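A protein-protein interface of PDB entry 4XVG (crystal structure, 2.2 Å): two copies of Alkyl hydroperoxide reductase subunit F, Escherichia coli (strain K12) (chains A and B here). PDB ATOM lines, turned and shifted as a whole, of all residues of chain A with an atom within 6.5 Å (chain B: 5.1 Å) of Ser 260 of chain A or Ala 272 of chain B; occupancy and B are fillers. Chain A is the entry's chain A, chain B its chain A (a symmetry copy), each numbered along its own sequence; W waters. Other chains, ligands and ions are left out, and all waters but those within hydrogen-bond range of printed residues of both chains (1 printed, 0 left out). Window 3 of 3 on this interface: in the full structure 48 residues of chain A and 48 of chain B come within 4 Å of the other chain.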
ATOM      1  N   ASN A 257     -26.194  17.881  29.120  1.00  0.00           N
ATOM      2  CA  ASN A 257     -24.880  17.428  28.667  1.00  0.00           C
ATOM      3  C   ASN A 257     -24.941  16.365  27.590  1.00  0.00           C
ATOM      4  O   ASN A 257     -23.975  15.628  27.389  1.00  0.00           O
ATOM      5  CB  ASN A 257     -24.022  16.917  29.838  1.00  0.00           C
ATOM      6  CG  ASN A 257     -24.678  15.760  30.592  1.00  0.00           C
ATOM      7  OD1 ASN A 257     -25.731  15.240  30.184  1.00  0.00           O
ATOM      8  ND2 ASN A 257     -24.055  15.348  31.695  1.00  0.00           N
ATOM      9  N   TYR A 258     -26.063  16.267  26.889  1.00  0.00           N
ATOM     10  CA  TYR A 258     -26.063  15.441  25.701  1.00  0.00           C
ATOM     11  C   TYR A 258     -25.442  16.253  24.559  1.00  0.00           C
ATOM     12  O   TYR A 258     -26.112  17.060  23.899  1.00  0.00           O
ATOM     13  CB  TYR A 258     -27.447  14.906  25.346  1.00  0.00           C
ATOM     14  CG  TYR A 258     -27.333  13.819  24.310  1.00  0.00           C
ATOM     15  CD1 TYR A 258     -26.887  12.543  24.664  1.00  0.00           C
ATOM     16  CD2 TYR A 258     -27.610  14.072  22.973  1.00  0.00           C
ATOM     17  CE1 TYR A 258     -26.748  11.534  23.713  1.00  0.00           C
ATOM     18  CE2 TYR A 258     -27.471  13.063  22.001  1.00  0.00           C
ATOM     19  CZ  TYR A 258     -27.037  11.803  22.384  1.00  0.00           C
ATOM     20  OH  TYR A 258     -26.902  10.796  21.448  1.00  0.00           O
ATOM     21  N   ILE A 259     -24.143  16.021  24.364  1.00  0.00           N
ATOM     22  CA  ILE A 259     -23.281  16.856  23.526  1.00  0.00           C
ATOM     23  C   ILE A 259     -23.932  17.337  22.221  1.00  0.00           C
ATOM     24  O   ILE A 259     -24.423  16.518  21.435  1.00  0.00           O
ATOM     25  CB  ILE A 259     -21.957  16.120  23.229  1.00  0.00           C
ATOM     26  CG1 ILE A 259     -21.250  15.783  24.545  1.00  0.00           C
ATOM     27  CG2 ILE A 259     -21.054  16.957  22.394  1.00  0.00           C
ATOM     28  CD1 ILE A 259     -20.982  16.990  25.459  1.00  0.00           C
ATOM     29  N   SER A 260     -23.926  18.669  22.037  1.00  0.00           N
ATOM     30  CA  SER A 260     -24.465  19.424  20.875  1.00  0.00           C
ATOM     31  C   SER A 260     -25.925  19.849  21.061  1.00  0.00           C
ATOM     32  O   SER A 260     -26.461  20.600  20.245  1.00  0.00           O
ATOM     33  CB  SER A 260     -24.285  18.706  19.527  1.00  0.00           C
ATOM     34  OG  SER A 260     -25.396  17.841  19.265  1.00  0.00           O
ATOM     35  N   VAL A 261     -26.552  19.376  22.140  1.00  0.00           N
ATOM     36  CA  VAL A 261     -27.918  19.752  22.495  1.00  0.00           C
ATOM     37  C   VAL A 261     -27.890  20.377  23.879  1.00  0.00           C
ATOM     38  O   VAL A 261     -27.870  19.646  24.877  1.00  0.00           O
ATOM     39  CB  VAL A 261     -28.805  18.505  22.588  1.00  0.00           C
ATOM     40  CG1 VAL A 261     -30.264  18.891  22.880  1.00  0.00           C
ATOM     41  CG2 VAL A 261     -28.695  17.684  21.317  1.00  0.00           C
ATOM     42  N   PRO A 262     -27.876  21.725  23.947  1.00  0.00           N
ATOM     43  CA  PRO A 262     -27.658  22.441  25.215  1.00  0.00           C
ATOM     44  C   PRO A 262     -28.660  22.041  26.306  1.00  0.00           C
ATOM     45  O   PRO A 262     -28.321  22.011  27.492  1.00  0.00           O
ATOM     46  CB  PRO A 262     -27.846  23.916  24.823  1.00  0.00           C
ATOM     47  CG  PRO A 262     -27.437  23.956  23.356  1.00  0.00           C
ATOM     48  CD  PRO A 262     -27.975  22.645  22.797  1.00  0.00           C
ATOM     49  N   ILE B 229     -16.969  20.623  27.435  1.00  0.00           N
ATOM     50  CA  ILE B 229     -18.264  20.753  28.088  1.00  0.00           C
ATOM     51  C   ILE B 229     -18.276  19.992  29.403  1.00  0.00           C
ATOM     52  O   ILE B 229     -18.653  20.543  30.443  1.00  0.00           O
ATOM     53  CB  ILE B 229     -19.364  20.207  27.169  1.00  0.00           C
ATOM     54  CG1 ILE B 229     -19.545  21.174  25.987  1.00  0.00           C
ATOM     55  CG2 ILE B 229     -20.671  19.980  27.944  1.00  0.00           C
ATOM     56  CD1 ILE B 229     -20.313  20.597  24.809  1.00  0.00           C
ATOM     57  N   TYR B 258     -25.783  10.496  13.915  1.00  0.00           N
ATOM     58  CA  TYR B 258     -25.539  11.101  15.206  1.00  0.00           C
ATOM     59  C   TYR B 258     -26.760  10.832  16.094  1.00  0.00           C
ATOM     60  O   TYR B 258     -27.770  11.548  16.040  1.00  0.00           O
ATOM     61  CB  TYR B 258     -25.204  12.587  15.116  1.00  0.00           C
ATOM     62  CG  TYR B 258     -24.659  13.077  16.431  1.00  0.00           C
ATOM     63  CD1 TYR B 258     -23.354  12.765  16.821  1.00  0.00           C
ATOM     64  CD2 TYR B 258     -25.456  13.796  17.313  1.00  0.00           C
ATOM     65  CE1 TYR B 258     -22.845  13.186  18.048  1.00  0.00           C
ATOM     66  CE2 TYR B 258     -24.955  14.225  18.557  1.00  0.00           C
ATOM     67  CZ  TYR B 258     -23.652  13.912  18.911  1.00  0.00           C
ATOM     68  OH  TYR B 258     -23.137  14.329  20.123  1.00  0.00           O
ATOM     69  N   LYS B 268     -23.585  22.554  10.283  1.00  0.00           N
ATOM     70  CA  LYS B 268     -24.602  22.831  11.305  1.00  0.00           C
ATOM     71  C   LYS B 268     -24.185  22.206  12.645  1.00  0.00           C
ATOM     72  O   LYS B 268     -24.170  22.882  13.683  1.00  0.00           O
ATOM     73  CB  LYS B 268     -25.981  22.318  10.842  1.00  0.00           C
ATOM     74  CG  LYS B 268     -27.080  22.332  11.922  1.00  0.00           C
ATOM     75  CD  LYS B 268     -28.511  22.323  11.324  1.00  0.00           C
ATOM     76  CE  LYS B 268     -28.724  21.180  10.319  1.00  0.00           C
ATOM     77  NZ  LYS B 268     -30.111  21.139   9.713  1.00  0.00           N
ATOM     78  N   LEU B 269     -23.809  20.930  12.611  1.00  0.00           N
ATOM     79  CA  LEU B 269     -23.372  20.223  13.816  1.00  0.00           C
ATOM     80  C   LEU B 269     -22.205  20.919  14.504  1.00  0.00           C
ATOM     81  O   LEU B 269     -22.206  21.052  15.730  1.00  0.00           O
ATOM     82  CB  LEU B 269     -23.027  18.765  13.495  1.00  0.00           C
ATOM     83  CG  LEU B 269     -22.539  17.864  14.646  1.00  0.00           C
ATOM     84  CD1 LEU B 269     -23.497  17.921  15.839  1.00  0.00           C
ATOM     85  CD2 LEU B 269     -22.387  16.426  14.156  1.00  0.00           C
ATOM     86  N   ALA B 270     -21.218  21.378  13.735  1.00  0.00           N
ATOM     87  CA  ALA B 270     -20.078  22.059  14.349  1.00  0.00           C
ATOM     88  C   ALA B 270     -20.535  23.351  15.003  1.00  0.00           C
ATOM     89  O   ALA B 270     -20.012  23.742  16.046  1.00  0.00           O
ATOM     90  CB  ALA B 270     -18.994  22.342  13.342  1.00  0.00           C
ATOM     91  N   GLY B 271     -21.509  24.013  14.388  1.00  0.00           N
ATOM     92  CA  GLY B 271     -22.067  25.222  14.967  1.00  0.00           C
ATOM     93  C   GLY B 271     -22.766  24.911  16.281  1.00  0.00           C
ATOM     94  O   GLY B 271     -22.691  25.682  17.248  1.00  0.00           O
ATOM     95  N   ALA B 272     -23.445  23.771  16.326  1.00  0.00           N
ATOM     96  CA  ALA B 272     -24.149  23.392  17.548  1.00  0.00           C
ATOM     97  C   ALA B 272     -23.145  23.035  18.650  1.00  0.00           C
ATOM     98  O   ALA B 272     -23.313  23.430  19.812  1.00  0.00           O
ATOM     99  CB  ALA B 272     -25.090  22.247  17.268  1.00  0.00           C
ATOM    100  N   LEU B 273     -22.090  22.308  18.288  1.00  0.00           N
ATOM    101  CA  LEU B 273     -21.028  22.004  19.247  1.00  0.00           C
ATOM    102  C   LEU B 273     -20.515  23.303  19.857  1.00  0.00           C
ATOM    103  O   LEU B 273     -20.388  23.424  21.082  1.00  0.00           O
ATOM    104  CB  LEU B 273     -19.877  21.230  18.581  1.00  0.00           C
ATOM    105  CG  LEU B 273     -20.178  19.772  18.203  1.00  0.00           C
ATOM    106  CD1 LEU B 273     -19.040  19.185  17.336  1.00  0.00           C
ATOM    107  CD2 LEU B 273     -20.359  18.922  19.465  1.00  0.00           C
ATOM    108  N   LYS B 274     -20.264  24.297  19.008  1.00  0.00           N
ATOM    109  CA  LYS B 274     -19.765  25.591  19.489  1.00  0.00           C
ATOM    110  C   LYS B 274     -20.722  26.275  20.468  1.00  0.00           C
ATOM    111  O   LYS B 274     -20.284  26.812  21.496  1.00  0.00           O
ATOM    112  CB  LYS B 274     -19.448  26.528  18.317  1.00  0.00           C
ATOM    113  CG  LYS B 274     -18.673  27.764  18.744  1.00  0.00           C
ATOM    114  CD  LYS B 274     -17.521  27.380  19.692  1.00  0.00           C
ATOM    115  CE  LYS B 274     -16.483  28.488  19.784  1.00  0.00           C
ATOM    116  NZ  LYS B 274     -17.074  29.835  19.551  1.00  0.00           N
ATOM    117  N   VAL B 275     -22.020  26.258  20.158  1.00  0.00           N
ATOM    118  CA  VAL B 275     -23.015  26.839  21.070  1.00  0.00           C
ATOM    119  C   VAL B 275     -22.995  26.119  22.417  1.00  0.00           C
ATOM    120  O   VAL B 275     -23.027  26.761  23.466  1.00  0.00           O
ATOM    121  CB  VAL B 275     -24.446  26.830  20.477  1.00  0.00           C
ATOM    122  CG1 VAL B 275     -25.497  27.063  21.573  1.00  0.00           C
ATOM    123  CG2 VAL B 275     -24.576  27.896  19.351  1.00  0.00           C
ATOM    124  N   HIS B 276     -22.914  24.789  22.382  1.00  0.00           N
ATOM    125  CA  HIS B 276     -22.921  23.996  23.612  1.00  0.00           C
ATOM    126  C   HIS B 276     -21.691  24.322  24.464  1.00  0.00           C
ATOM    127  O   HIS B 276     -21.811  24.588  25.672  1.00  0.00           O
ATOM    128  CB  HIS B 276     -23.019  22.494  23.321  1.00  0.00           C
ATOM    129  CG  HIS B 276     -23.637  21.700  24.444  1.00  0.00           C
ATOM    130  ND1 HIS B 276     -24.038  20.388  24.295  1.00  0.00           N
ATOM    131  CD2 HIS B 276     -23.927  22.038  25.721  1.00  0.00           C
ATOM    132  CE1 HIS B 276     -24.533  19.946  25.439  1.00  0.00           C
ATOM    133  NE2 HIS B 276     -24.478  20.923  26.324  1.00  0.00           N
ATOM    134  N   VAL B 277     -20.525  24.338  23.828  1.00  0.00           N
ATOM    135  CA  VAL B 277     -19.294  24.745  24.495  1.00  0.00           C
ATOM    136  C   VAL B 277     -19.390  26.133  25.138  1.00  0.00           C
ATOM    137  O   VAL B 277     -19.020  26.308  26.312  1.00  0.00           O
ATOM    138  CB  VAL B 277     -18.077  24.697  23.523  1.00  0.00           C
ATOM    139  CG1 VAL B 277     -16.825  25.235  24.207  1.00  0.00           C
ATOM    140  CG2 VAL B 277     -17.825  23.258  23.043  1.00  0.00           C
HETATM  141  O   HOH W   1     -25.930  23.063  28.117  1.00  0.00           O
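O of Ile 259 of chain A is in hydrogen-bond range of OH of Tyr 258 of chain B (2.9 Å).
The backbone NH (N) of Ser 260 of chain A is in hydrogen-bond range of a ring nitrogen (ND1) of His 276 of chain B.
ND1 of His 276 of chain B is in hydrogen-bond range of N of Val 261 of chain A (3.5 Å).
Printed residues of chain A that touch a printed residue of chain B: Tyr 258, Ile 259, Ser 260, Val 261 and Pro 262.
Hydrophobic or aromatic side chains of chain A within 4 Å of the printed part of chain B: Ile 259.
Printed residues of chain B that touch a printed residue of chain A: Ile 229, Tyr 258, Leu 269, Ala 272, Leu 273 and His 276.
Hydrophobic or aromatic side chains of chain B that line the printed part of chain A: Ile 229, Tyr 258, Leu 269, Ala 272, Leu 273 and His 276.
Position printed for both chains: 258.
Ser 260 of chain A touches five residues of chain B.
Of chain A, only Ser 260 comes within 4 Å of Ala 272 of chain B.
Printed residues of chain B within 4 Å of Val 261 of chain A: His 276 (3.4 Å).
Printed residues of chain A within 4 Å of Leu 273 of chain B: Ile 259 (3.6 Å) and Ser 260 (3.9 Å).
Of the printed residues of chain B, Pro 262 of chain A touches His 276 (3.7 Å).
Of the printed residues of chain A, Ile 229 of chain B touches Ile 259 (3.7 Å).
The nearest residue of chain B that does not touch Ser 260 of chain A is Ile 229 of chain B (4.9 Å).
Tyr 258 of chain A touches His 276 of chain B.
Ile 229 of chain B touches Ile 259 of chain A.
CD2 of Leu 273 of chain B touches CG2 of Ile 259 of chain A, at 3.6 Å.
C of Ile 259 of chain A touches ND1 of His 276 of chain B, 3.7 Å away.
Tyr 258 of chain B touches Ser 260 of chain A.
Ser 260 of chain A touches Leu 269 of chain B (CB to CD1, 3.9 Å).
Ser 260 of chain A touches Ala 272 of chain B.
CB of Ser 260 of chain A touches CD2 of Leu 273 of chain B (3.9 Å).
Pro 262 of chain A touches His 276 of chain B (CA to NE2, 3.7 Å).
Water W1 lies within hydrogen-bond range of O of Pro 262 of chain A (2.7 Å) and NE2 of His 276 of chain B (3.1 Å).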
